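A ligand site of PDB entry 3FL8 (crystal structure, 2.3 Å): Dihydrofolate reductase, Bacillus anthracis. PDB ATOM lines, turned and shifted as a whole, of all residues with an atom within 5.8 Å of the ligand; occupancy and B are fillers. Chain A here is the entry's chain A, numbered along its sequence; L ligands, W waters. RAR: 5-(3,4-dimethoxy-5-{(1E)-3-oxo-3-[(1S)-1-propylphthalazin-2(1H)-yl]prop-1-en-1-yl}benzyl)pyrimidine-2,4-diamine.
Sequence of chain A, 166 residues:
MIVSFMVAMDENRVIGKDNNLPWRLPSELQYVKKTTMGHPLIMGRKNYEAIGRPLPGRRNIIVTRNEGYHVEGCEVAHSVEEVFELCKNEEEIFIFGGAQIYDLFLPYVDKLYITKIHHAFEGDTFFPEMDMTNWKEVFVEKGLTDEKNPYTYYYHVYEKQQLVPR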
ATOM      1  N   MET A   6      28.264   9.342 -31.011  1.00  0.00           N
ATOM      2  CA  MET A   6      27.387   9.727 -29.913  1.00  0.00           C
ATOM      3  C   MET A   6      27.080   8.463 -29.144  1.00  0.00           C
ATOM      4  O   MET A   6      26.518   7.524 -29.689  1.00  0.00           O
ATOM      5  CB  MET A   6      26.102  10.373 -30.445  1.00  0.00           C
ATOM      6  CG  MET A   6      24.996  10.556 -29.435  1.00  0.00           C
ATOM      7  SD  MET A   6      25.406  11.665 -28.072  1.00  0.00           S
ATOM      8  CE  MET A   6      25.560  13.253 -28.881  1.00  0.00           C
ATOM      9  N   VAL A   7      27.491   8.402 -27.889  1.00  0.00           N
ATOM     10  CA  VAL A   7      27.296   7.167 -27.134  1.00  0.00           C
ATOM     11  C   VAL A   7      27.021   7.383 -25.637  1.00  0.00           C
ATOM     12  O   VAL A   7      27.537   8.339 -25.012  1.00  0.00           O
ATOM     13  CB  VAL A   7      28.480   6.191 -27.332  1.00  0.00           C
ATOM     14  CG1 VAL A   7      29.748   6.760 -26.764  1.00  0.00           C
ATOM     15  CG2 VAL A   7      28.194   4.857 -26.689  1.00  0.00           C
ATOM     16  N   ALA A   8      26.190   6.514 -25.086  1.00  0.00           N
ATOM     17  CA  ALA A   8      26.008   6.451 -23.658  1.00  0.00           C
ATOM     18  C   ALA A   8      26.356   5.040 -23.233  1.00  0.00           C
ATOM     19  O   ALA A   8      25.861   4.089 -23.823  1.00  0.00           O
ATOM     20  CB  ALA A   8      24.563   6.786 -23.281  1.00  0.00           C
ATOM     21  N   ILE A  15      26.369  -0.784 -23.779  1.00  0.00           N
ATOM     22  CA  ILE A  15      25.545   0.197 -24.476  1.00  0.00           C
ATOM     23  C   ILE A  15      24.158  -0.379 -24.776  1.00  0.00           C
ATOM     24  O   ILE A  15      23.324   0.311 -25.359  1.00  0.00           O
ATOM     25  CB  ILE A  15      26.195   0.650 -25.792  1.00  0.00           C
ATOM     26  CG1 ILE A  15      26.464  -0.551 -26.703  1.00  0.00           C
ATOM     27  CG2 ILE A  15      27.498   1.404 -25.526  1.00  0.00           C
ATOM     28  CD1 ILE A  15      26.984  -0.175 -28.092  1.00  0.00           C
ATOM     29  N   ASN A  19      18.605  -5.314 -26.484  1.00  0.00           N
ATOM     30  CA  ASN A  19      18.374  -4.391 -27.583  1.00  0.00           C
ATOM     31  C   ASN A  19      18.017  -2.991 -27.087  1.00  0.00           C
ATOM     32  O   ASN A  19      18.149  -2.017 -27.823  1.00  0.00           O
ATOM     33  CB  ASN A  19      17.261  -4.919 -28.497  1.00  0.00           C
ATOM     34  CG  ASN A  19      17.796  -5.402 -29.838  1.00  0.00           C
ATOM     35  OD1 ASN A  19      18.896  -5.048 -30.242  1.00  0.00           O
ATOM     36  ND2 ASN A  19      17.002  -6.216 -30.531  1.00  0.00           N
ATOM     37  N   ASN A  20      17.569  -2.904 -25.847  1.00  0.00           N
ATOM     38  CA  ASN A  20      17.200  -1.636 -25.261  1.00  0.00           C
ATOM     39  C   ASN A  20      18.286  -1.112 -24.328  1.00  0.00           C
ATOM     40  O   ASN A  20      19.328  -1.746 -24.141  1.00  0.00           O
ATOM     41  CB  ASN A  20      15.861  -1.762 -24.532  1.00  0.00           C
ATOM     42  CG  ASN A  20      14.686  -1.655 -25.483  1.00  0.00           C
ATOM     43  OD1 ASN A  20      14.632  -0.752 -26.323  1.00  0.00           O
ATOM     44  ND2 ASN A  20      13.734  -2.575 -25.366  1.00  0.00           N
ATOM     45  N   LEU A  21      18.053   0.074 -23.769  1.00  0.00           N
ATOM     46  CA  LEU A  21      18.965   0.650 -22.800  1.00  0.00           C
ATOM     47  C   LEU A  21      18.649   0.059 -21.430  1.00  0.00           C
ATOM     48  O   LEU A  21      17.493   0.056 -21.009  1.00  0.00           O
ATOM     49  CB  LEU A  21      18.802   2.160 -22.746  1.00  0.00           C
ATOM     50  CG  LEU A  21      19.128   2.945 -24.001  1.00  0.00           C
ATOM     51  CD1 LEU A  21      18.755   4.413 -23.806  1.00  0.00           C
ATOM     52  CD2 LEU A  21      20.604   2.793 -24.345  1.00  0.00           C
ATOM     53  N   PRO A  26      15.898  10.074 -18.977  1.00  0.00           N
ATOM     54  CA  PRO A  26      15.254  11.050 -19.862  1.00  0.00           C
ATOM     55  C   PRO A  26      16.145  12.279 -20.097  1.00  0.00           C
ATOM     56  O   PRO A  26      16.211  12.806 -21.212  1.00  0.00           O
ATOM     57  CB  PRO A  26      14.011  11.486 -19.080  1.00  0.00           C
ATOM     58  CG  PRO A  26      13.771  10.394 -18.097  1.00  0.00           C
ATOM     59  CD  PRO A  26      15.063   9.714 -17.822  1.00  0.00           C
ATOM     60  N   GLU A  28      19.399  12.444 -20.060  1.00  0.00           N
ATOM     61  CA  GLU A  28      20.478  12.072 -20.984  1.00  0.00           C
ATOM     62  C   GLU A  28      19.975  12.186 -22.435  1.00  0.00           C
ATOM     63  O   GLU A  28      20.620  12.800 -23.279  1.00  0.00           O
ATOM     64  CB  GLU A  28      21.000  10.657 -20.694  1.00  0.00           C
ATOM     65  CG  GLU A  28      22.441  10.404 -21.107  1.00  0.00           C
ATOM     66  CD  GLU A  28      22.625  10.095 -22.587  1.00  0.00           C
ATOM     67  OE1 GLU A  28      21.798   9.352 -23.161  1.00  0.00           O
ATOM     68  OE2 GLU A  28      23.624  10.571 -23.169  1.00  0.00           O
ATOM     69  N   LEU A  29      18.811  11.598 -22.714  1.00  0.00           N
ATOM     70  CA  LEU A  29      18.232  11.630 -24.045  1.00  0.00           C
ATOM     71  C   LEU A  29      17.959  13.065 -24.516  1.00  0.00           C
ATOM     72  O   LEU A  29      18.080  13.366 -25.690  1.00  0.00           O
ATOM     73  CB  LEU A  29      16.969  10.783 -24.094  1.00  0.00           C
ATOM     74  CG  LEU A  29      17.240   9.310 -23.792  1.00  0.00           C
ATOM     75  CD1 LEU A  29      15.979   8.459 -23.932  1.00  0.00           C
ATOM     76  CD2 LEU A  29      18.342   8.781 -24.702  1.00  0.00           C
ATOM     77  N   GLN A  30      17.597  13.946 -23.588  1.00  0.00           N
ATOM     78  CA  GLN A  30      17.381  15.352 -23.903  1.00  0.00           C
ATOM     79  C   GLN A  30      18.697  16.000 -24.282  1.00  0.00           C
ATOM     80  O   GLN A  30      18.725  16.908 -25.121  1.00  0.00           O
ATOM     81  CB  GLN A  30      16.772  16.067 -22.699  1.00  0.00           C
ATOM     82  CG  GLN A  30      15.926  17.252 -23.067  1.00  0.00           C
ATOM     83  CD  GLN A  30      14.689  16.854 -23.859  1.00  0.00           C
ATOM     84  OE1 GLN A  30      14.154  15.753 -23.705  1.00  0.00           O
ATOM     85  NE2 GLN A  30      14.232  17.759 -24.718  1.00  0.00           N
ATOM     86  N   TYR A  31      19.786  15.562 -23.658  1.00  0.00           N
ATOM     87  CA  TYR A  31      21.113  16.013 -24.058  1.00  0.00           C
ATOM     88  C   TYR A  31      21.422  15.556 -25.488  1.00  0.00           C
ATOM     89  O   TYR A  31      21.914  16.342 -26.290  1.00  0.00           O
ATOM     90  CB  TYR A  31      22.182  15.501 -23.097  1.00  0.00           C
ATOM     91  CG  TYR A  31      23.609  15.718 -23.578  1.00  0.00           C
ATOM     92  CD1 TYR A  31      24.263  16.923 -23.336  1.00  0.00           C
ATOM     93  CD2 TYR A  31      24.307  14.725 -24.239  1.00  0.00           C
ATOM     94  CE1 TYR A  31      25.568  17.134 -23.760  1.00  0.00           C
ATOM     95  CE2 TYR A  31      25.608  14.921 -24.656  1.00  0.00           C
ATOM     96  CZ  TYR A  31      26.232  16.125 -24.419  1.00  0.00           C
ATOM     97  OH  TYR A  31      27.530  16.325 -24.814  1.00  0.00           O
ATOM     98  N   VAL A  32      21.132  14.298 -25.786  1.00  0.00           N
ATOM     99  CA  VAL A  32      21.308  13.781 -27.126  1.00  0.00           C
ATOM    100  C   VAL A  32      20.544  14.663 -28.117  1.00  0.00           C
ATOM    101  O   VAL A  32      21.107  15.126 -29.121  1.00  0.00           O
ATOM    102  CB  VAL A  32      20.832  12.330 -27.255  1.00  0.00           C
ATOM    103  CG1 VAL A  32      20.782  11.913 -28.710  1.00  0.00           C
ATOM    104  CG2 VAL A  32      21.734  11.411 -26.436  1.00  0.00           C
ATOM    105  N   LYS A  33      19.271  14.930 -27.815  1.00  0.00           N
ATOM    106  CA  LYS A  33      18.435  15.726 -28.708  1.00  0.00           C
ATOM    107  C   LYS A  33      19.014  17.128 -28.921  1.00  0.00           C
ATOM    108  O   LYS A  33      19.082  17.607 -30.053  1.00  0.00           O
ATOM    109  CB  LYS A  33      17.015  15.832 -28.177  1.00  0.00           C
ATOM    110  CG  LYS A  33      16.091  16.669 -29.044  1.00  0.00           C
ATOM    111  CD  LYS A  33      14.672  16.701 -28.488  1.00  0.00           C
ATOM    112  CE  LYS A  33      13.776  17.622 -29.316  1.00  0.00           C
ATOM    113  NZ  LYS A  33      12.416  17.675 -28.735  1.00  0.00           N
ATOM    114  N   THR A  36      22.444  16.909 -31.098  1.00  0.00           N
ATOM    115  CA  THR A  36      22.399  16.427 -32.477  1.00  0.00           C
ATOM    116  C   THR A  36      21.424  17.214 -33.357  1.00  0.00           C
ATOM    117  O   THR A  36      21.175  16.830 -34.503  1.00  0.00           O
ATOM    118  CB  THR A  36      21.958  14.958 -32.554  1.00  0.00           C
ATOM    119  OG1 THR A  36      20.706  14.816 -31.894  1.00  0.00           O
ATOM    120  CG2 THR A  36      22.986  14.045 -31.917  1.00  0.00           C
ATOM    121  N   LEU A  41      21.610  11.695 -38.012  1.00  0.00           N
ATOM    122  CA  LEU A  41      21.824  10.592 -37.087  1.00  0.00           C
ATOM    123  C   LEU A  41      22.073   9.333 -37.878  1.00  0.00           C
ATOM    124  O   LEU A  41      21.221   8.925 -38.662  1.00  0.00           O
ATOM    125  CB  LEU A  41      20.585  10.365 -36.234  1.00  0.00           C
ATOM    126  CG  LEU A  41      20.325  11.367 -35.127  1.00  0.00           C
ATOM    127  CD1 LEU A  41      19.147  10.875 -34.301  1.00  0.00           C
ATOM    128  CD2 LEU A  41      21.575  11.489 -34.274  1.00  0.00           C
ATOM    129  N   ASN A  47      19.490  -0.896 -34.073  1.00  0.00           N
ATOM    130  CA  ASN A  47      19.491   0.283 -33.209  1.00  0.00           C
ATOM    131  C   ASN A  47      18.257   1.125 -33.498  1.00  0.00           C
ATOM    132  O   ASN A  47      17.580   1.569 -32.579  1.00  0.00           O
ATOM    133  CB  ASN A  47      20.778   1.096 -33.418  1.00  0.00           C
ATOM    134  CG  ASN A  47      21.166   1.912 -32.178  1.00  0.00           C
ATOM    135  OD1 ASN A  47      21.428   1.358 -31.113  1.00  0.00           O
ATOM    136  ND2 ASN A  47      21.211   3.227 -32.324  1.00  0.00           N
ATOM    137  N   ALA A  50      15.137  -0.542 -32.156  1.00  0.00           N
ATOM    138  CA  ALA A  50      15.069  -0.445 -30.699  1.00  0.00           C
ATOM    139  C   ALA A  50      14.482   0.888 -30.227  1.00  0.00           C
ATOM    140  O   ALA A  50      13.846   0.965 -29.187  1.00  0.00           O
ATOM    141  CB  ALA A  50      16.441  -0.636 -30.111  1.00  0.00           C
ATOM    142  N   ILE A  51      14.673   1.936 -31.023  1.00  0.00           N
ATOM    143  CA  ILE A  51      14.158   3.262 -30.709  1.00  0.00           C
ATOM    144  C   ILE A  51      12.692   3.424 -31.145  1.00  0.00           C
ATOM    145  O   ILE A  51      11.949   4.207 -30.551  1.00  0.00           O
ATOM    146  CB  ILE A  51      15.022   4.359 -31.372  1.00  0.00           C
ATOM    147  CG1 ILE A  51      16.465   4.255 -30.881  1.00  0.00           C
ATOM    148  CG2 ILE A  51      14.446   5.738 -31.107  1.00  0.00           C
ATOM    149  CD1 ILE A  51      17.423   5.217 -31.568  1.00  0.00           C
ATOM    150  N   ARG A  53      10.894   4.863 -33.545  1.00  0.00           N
ATOM    151  CA  ARG A  53      10.390   5.911 -34.434  1.00  0.00           C
ATOM    152  C   ARG A  53      11.523   6.776 -34.989  1.00  0.00           C
ATOM    153  O   ARG A  53      12.601   6.825 -34.394  1.00  0.00           O
ATOM    154  CB  ARG A  53       9.412   6.813 -33.666  1.00  0.00           C
ATOM    155  CG  ARG A  53      10.098   7.633 -32.582  1.00  0.00           C
ATOM    156  CD  ARG A  53       9.099   8.249 -31.624  1.00  0.00           C
ATOM    157  NE  ARG A  53       9.771   8.841 -30.475  1.00  0.00           N
ATOM    158  CZ  ARG A  53      10.086  10.130 -30.379  1.00  0.00           C
ATOM    159  NH1 ARG A  53       9.795  10.972 -31.361  1.00  0.00           N
ATOM    160  NH2 ARG A  53      10.698  10.575 -29.286  1.00  0.00           N
ATOM    161  N   LEU A  55      13.542   9.910 -35.147  1.00  0.00           N
ATOM    162  CA  LEU A  55      13.726  11.023 -34.235  1.00  0.00           C
ATOM    163  C   LEU A  55      13.577  12.327 -35.013  1.00  0.00           C
ATOM    164  O   LEU A  55      14.403  12.653 -35.866  1.00  0.00           O
ATOM    165  CB  LEU A  55      15.084  10.927 -33.549  1.00  0.00           C
ATOM    166  CG  LEU A  55      15.261   9.612 -32.791  1.00  0.00           C
ATOM    167  CD1 LEU A  55      16.609   9.547 -32.072  1.00  0.00           C
ATOM    168  CD2 LEU A  55      14.110   9.389 -31.807  1.00  0.00           C
ATOM    169  N   PRO A  56      12.481  13.063 -34.730  1.00  0.00           N
ATOM    170  CA  PRO A  56      12.096  14.253 -35.496  1.00  0.00           C
ATOM    171  C   PRO A  56      13.196  15.311 -35.498  1.00  0.00           C
ATOM    172  O   PRO A  56      13.991  15.385 -34.562  1.00  0.00           O
ATOM    173  CB  PRO A  56      10.870  14.770 -34.727  1.00  0.00           C
ATOM    174  CG  PRO A  56      10.332  13.565 -34.023  1.00  0.00           C
ATOM    175  CD  PRO A  56      11.543  12.768 -33.636  1.00  0.00           C
ATOM    176  N   ARG A  58      15.755  15.628 -37.536  1.00  0.00           N
ATOM    177  CA  ARG A  58      17.058  15.194 -38.052  1.00  0.00           C
ATOM    178  C   ARG A  58      16.887  14.256 -39.244  1.00  0.00           C
ATOM    179  O   ARG A  58      15.888  13.545 -39.356  1.00  0.00           O
ATOM    180  CB  ARG A  58      17.868  14.455 -36.981  1.00  0.00           C
ATOM    181  CG  ARG A  58      18.316  15.297 -35.820  1.00  0.00           C
ATOM    182  CD  ARG A  58      17.637  14.875 -34.539  1.00  0.00           C
ATOM    183  NE  ARG A  58      17.913  15.823 -33.460  1.00  0.00           N
ATOM    184  CZ  ARG A  58      17.150  16.877 -33.186  1.00  0.00           C
ATOM    185  NH1 ARG A  58      16.043  17.116 -33.883  1.00  0.00           N
ATOM    186  NH2 ARG A  58      17.472  17.695 -32.191  1.00  0.00           N
ATOM    187  N   ILE A  95      27.301   9.275 -35.458  1.00  0.00           N
ATOM    188  CA  ILE A  95      27.175   7.840 -35.503  1.00  0.00           C
ATOM    189  C   ILE A  95      26.501   7.459 -34.202  1.00  0.00           C
ATOM    190  O   ILE A  95      27.048   7.658 -33.111  1.00  0.00           O
ATOM    191  CB  ILE A  95      28.522   7.163 -35.612  1.00  0.00           C
ATOM    192  CG1 ILE A  95      29.335   7.811 -36.738  1.00  0.00           C
ATOM    193  CG2 ILE A  95      28.355   5.680 -35.872  1.00  0.00           C
ATOM    194  CD1 ILE A  95      28.628   7.837 -38.073  1.00  0.00           C
ATOM    195  N   PHE A  96      25.293   6.921 -34.314  1.00  0.00           N
ATOM    196  CA  PHE A  96      24.403   6.779 -33.159  1.00  0.00           C
ATOM    197  C   PHE A  96      24.456   5.392 -32.586  1.00  0.00           C
ATOM    198  O   PHE A  96      23.765   5.068 -31.611  1.00  0.00           O
ATOM    199  CB  PHE A  96      22.974   7.145 -33.557  1.00  0.00           C
ATOM    200  CG  PHE A  96      22.137   7.613 -32.413  1.00  0.00           C
ATOM    201  CD1 PHE A  96      22.552   8.666 -31.622  1.00  0.00           C
ATOM    202  CD2 PHE A  96      20.924   7.004 -32.144  1.00  0.00           C
ATOM    203  CE1 PHE A  96      21.776   9.106 -30.586  1.00  0.00           C
ATOM    204  CE2 PHE A  96      20.147   7.444 -31.109  1.00  0.00           C
ATOM    205  CZ  PHE A  96      20.585   8.499 -30.328  1.00  0.00           C
ATOM    206  N   GLY A  97      25.240   4.544 -33.224  1.00  0.00           N
ATOM    207  CA  GLY A  97      25.486   3.253 -32.644  1.00  0.00           C
ATOM    208  C   GLY A  97      24.860   2.054 -33.309  1.00  0.00           C
ATOM    209  O   GLY A  97      24.250   2.127 -34.385  1.00  0.00           O
ATOM    210  N   TYR A 102      29.711   1.504 -35.017  1.00  0.00           N
ATOM    211  CA  TYR A 102      30.839   2.262 -34.501  1.00  0.00           C
ATOM    212  C   TYR A 102      32.103   1.718 -35.137  1.00  0.00           C
ATOM    213  O   TYR A 102      32.981   2.479 -35.527  1.00  0.00           O
ATOM    214  CB  TYR A 102      30.952   2.184 -32.977  1.00  0.00           C
ATOM    215  CG  TYR A 102      29.864   2.895 -32.219  1.00  0.00           C
ATOM    216  CD1 TYR A 102      29.615   4.252 -32.432  1.00  0.00           C
ATOM    217  CD2 TYR A 102      29.088   2.232 -31.259  1.00  0.00           C
ATOM    218  CE1 TYR A 102      28.614   4.933 -31.744  1.00  0.00           C
ATOM    219  CE2 TYR A 102      28.101   2.904 -30.552  1.00  0.00           C
ATOM    220  CZ  TYR A 102      27.862   4.244 -30.797  1.00  0.00           C
ATOM    221  OH  TYR A 102      26.876   4.897 -30.105  1.00  0.00           O
ATOM    222  N   TYR A 113      31.406  12.075 -28.378  1.00  0.00           N
ATOM    223  CA  TYR A 113      30.473  12.508 -27.352  1.00  0.00           C
ATOM    224  C   TYR A 113      30.072  11.299 -26.547  1.00  0.00           C
ATOM    225  O   TYR A 113      29.250  10.498 -26.988  1.00  0.00           O
ATOM    226  CB  TYR A 113      29.220  13.117 -27.986  1.00  0.00           C
ATOM    227  CG  TYR A 113      29.463  14.359 -28.841  1.00  0.00           C
ATOM    228  CD1 TYR A 113      30.020  14.247 -30.116  1.00  0.00           C
ATOM    229  CD2 TYR A 113      29.140  15.622 -28.380  1.00  0.00           C
ATOM    230  CE1 TYR A 113      30.237  15.365 -30.899  1.00  0.00           C
ATOM    231  CE2 TYR A 113      29.358  16.746 -29.150  1.00  0.00           C
ATOM    232  CZ  TYR A 113      29.902  16.602 -30.402  1.00  0.00           C
ATOM    233  OH  TYR A 113      30.098  17.704 -31.177  1.00  0.00           O
ATOM    234  N   THR A 115      28.707   9.677 -22.965  1.00  0.00           N
ATOM    235  CA  THR A 115      28.103   9.760 -21.651  1.00  0.00           C
ATOM    236  C   THR A 115      28.539   8.541 -20.860  1.00  0.00           C
ATOM    237  O   THR A 115      28.272   7.409 -21.254  1.00  0.00           O
ATOM    238  CB  THR A 115      26.552   9.781 -21.693  1.00  0.00           C
ATOM    239  OG1 THR A 115      26.090  10.902 -22.454  1.00  0.00           O
ATOM    240  CG2 THR A 115      25.990   9.879 -20.295  1.00  0.00           C
HETATM  241  N01 RAR L   1      23.989   6.365 -29.156  1.00  0.00           N
HETATM  242  C02 RAR L   1      23.424   6.907 -28.032  1.00  0.00           C
HETATM  243  C03 RAR L   1      22.098   6.376 -27.620  1.00  0.00           C
HETATM  244  C04 RAR L   1      21.415   5.322 -28.470  1.00  0.00           C
HETATM  245  C05 RAR L   1      19.935   5.215 -28.166  1.00  0.00           C
HETATM  246  C06 RAR L   1      19.370   3.831 -27.791  1.00  0.00           C
HETATM  247  C07 RAR L   1      17.914   3.698 -27.431  1.00  0.00           C
HETATM  248  O08 RAR L   1      17.457   2.433 -27.117  1.00  0.00           O
HETATM  249  C09 RAR L   1      18.389   1.454 -27.273  1.00  0.00           C
HETATM  250  C10 RAR L   1      17.013   4.945 -27.427  1.00  0.00           C
HETATM  251  O11 RAR L   1      15.716   4.745 -27.032  1.00  0.00           O
HETATM  252  C12 RAR L   1      15.482   4.401 -25.662  1.00  0.00           C
HETATM  253  C13 RAR L   1      17.561   6.347 -27.785  1.00  0.00           C
HETATM  254  C14 RAR L   1      16.705   7.619 -27.787  1.00  0.00           C
HETATM  255  C15 RAR L   1      15.402   7.614 -27.796  1.00  0.00           C
HETATM  256  C16 RAR L   1      14.587   8.888 -27.671  1.00  0.00           C
HETATM  257  N17 RAR L   1      15.165  10.118 -28.071  1.00  0.00           N
HETATM  258  N18 RAR L   1      16.531  10.033 -28.491  1.00  0.00           N
HETATM  259  C19 RAR L   1      17.197  11.248 -28.774  1.00  0.00           C
HETATM  260  C20 RAR L   1      14.438  11.415 -28.101  1.00  0.00           C
HETATM  261  C21 RAR L   1      14.884  12.502 -27.033  1.00  0.00           C
HETATM  262  C22 RAR L   1      13.641  13.051 -26.362  1.00  0.00           C
HETATM  263  C23 RAR L   1      12.737  11.897 -25.973  1.00  0.00           C
HETATM  264  C24 RAR L   1      14.951  12.203 -29.354  1.00  0.00           C
HETATM  265  C25 RAR L   1      16.381  12.108 -29.658  1.00  0.00           C
HETATM  266  C26 RAR L   1      16.965  12.838 -30.867  1.00  0.00           C
HETATM  267  C27 RAR L   1      16.001  13.660 -31.678  1.00  0.00           C
HETATM  268  C28 RAR L   1      14.562  13.758 -31.344  1.00  0.00           C
HETATM  269  C29 RAR L   1      13.979  13.041 -30.179  1.00  0.00           C
HETATM  270  O30 RAR L   1      13.492   8.851 -27.300  1.00  0.00           O
HETATM  271  C31 RAR L   1      19.035   6.468 -28.149  1.00  0.00           C
HETATM  272  C32 RAR L   1      21.488   6.940 -26.403  1.00  0.00           C
HETATM  273  N33 RAR L   1      22.198   7.943 -25.718  1.00  0.00           N
HETATM  274  C34 RAR L   1      23.534   8.477 -26.148  1.00  0.00           C
HETATM  275  N35 RAR L   1      24.160   9.499 -25.427  1.00  0.00           N
HETATM  276  N36 RAR L   1      24.134   7.929 -27.333  1.00  0.00           N
HETATM  277  O   HOH W   1      12.523   5.089 -27.772  1.00  0.00           O
HETATM  278  O   HOH W   2      11.435  15.281 -26.031  1.00  0.00           O
HETATM  279  O   HOH W   3      14.989   1.638 -23.625  1.00  0.00           O
HETATM  280  O   HOH W   4      11.630   7.334 -29.290  1.00  0.00           O
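N of Thr 115 is in hydrogen-bond range of O of Val 7, 2.7 Å away. ND2 of Asn 47 sits at hydrogen-bond distance from O of Phe 96, at 3.2 Å. N of Met 6 sits at hydrogen-bond distance from O of Ile 95. OE2 of Glu 28 is in hydrogen-bond range of OG1 of Thr 115, 2.6 Å away. The backbone carbonyl oxygen (O) of Val 32 sits at hydrogen-bond distance from the side-chain hydroxyl (OG1) of Thr 36 (2.8 Å). NH2 of Arg 58 sits at hydrogen-bond distance from O of Lys 33, at 2.7 Å. The backbone carbonyl oxygen of Met 6 sits at hydrogen-bond distance from the side-chain hydroxyl of Tyr 102 (2.7 Å). O of Tyr 113 lies within hydrogen-bond range of N of Val 7 (2.9 Å).
Asn 19 touches the ligand. CA of Asn 20 touches C09 of the ligand, 3.9 Å away. CG of Leu 21 touches O08 of the ligand, at 3.6 Å. Leu 29 touches the ligand (O to C21, 3.6 Å). Gln 30 touches the ligand (OE1 to C22, 3.8 Å). Val 32 touches the ligand (CG2 to N35, 3.2 Å). Lys 33 touches the ligand. Ile 51 touches the ligand (CG1 to C10, 3.6 Å). Arg 53 touches the ligand. Leu 55 touches the ligand. Pro 56 touches the ligand (O to C28, 3.7 Å). Arg 58 touches the ligand (NE to C27, 3.4 Å). OG1 of Thr 115 touches N35 of the ligand, 3.8 Å away. Of the 29 residues printed, 19 come within 4 Å of the ligand. The nearest printed residue that does not touch the ligand is Ala 50 (4.03 Å).
N of Ala 8 lies within hydrogen-bond range of N36 of the ligand (3.4 Å). N of Val 7 lies close to N36 of the ligand, at 3.4 Å. The side-chain carboxylate of Glu 28 is in hydrogen-bond range of a nitrogen (N35) of the ligand (2.6 Å). OH of Tyr 102 lies within hydrogen-bond range of N01 of the ligand. N01 of the ligand lies within hydrogen-bond range of O of Met 6 (2.8 Å). The side-chain sulfur of Met 6 is in hydrogen-bond range of a nitrogen (N35) of the ligand. The backbone carbonyl oxygen of Phe 96 lies within hydrogen-bond range of a nitrogen (N01) of the ligand, at 2.8 Å.
Water W4 lies within hydrogen-bond range of the guanidinium group of Arg 53, an oxygen (O30) of the ligand and the backbone carbonyl oxygen of Ile 51. Water W1 bridges the backbone carbonyl oxygen of Ile 51 and an oxygen (O11) of the ligand.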
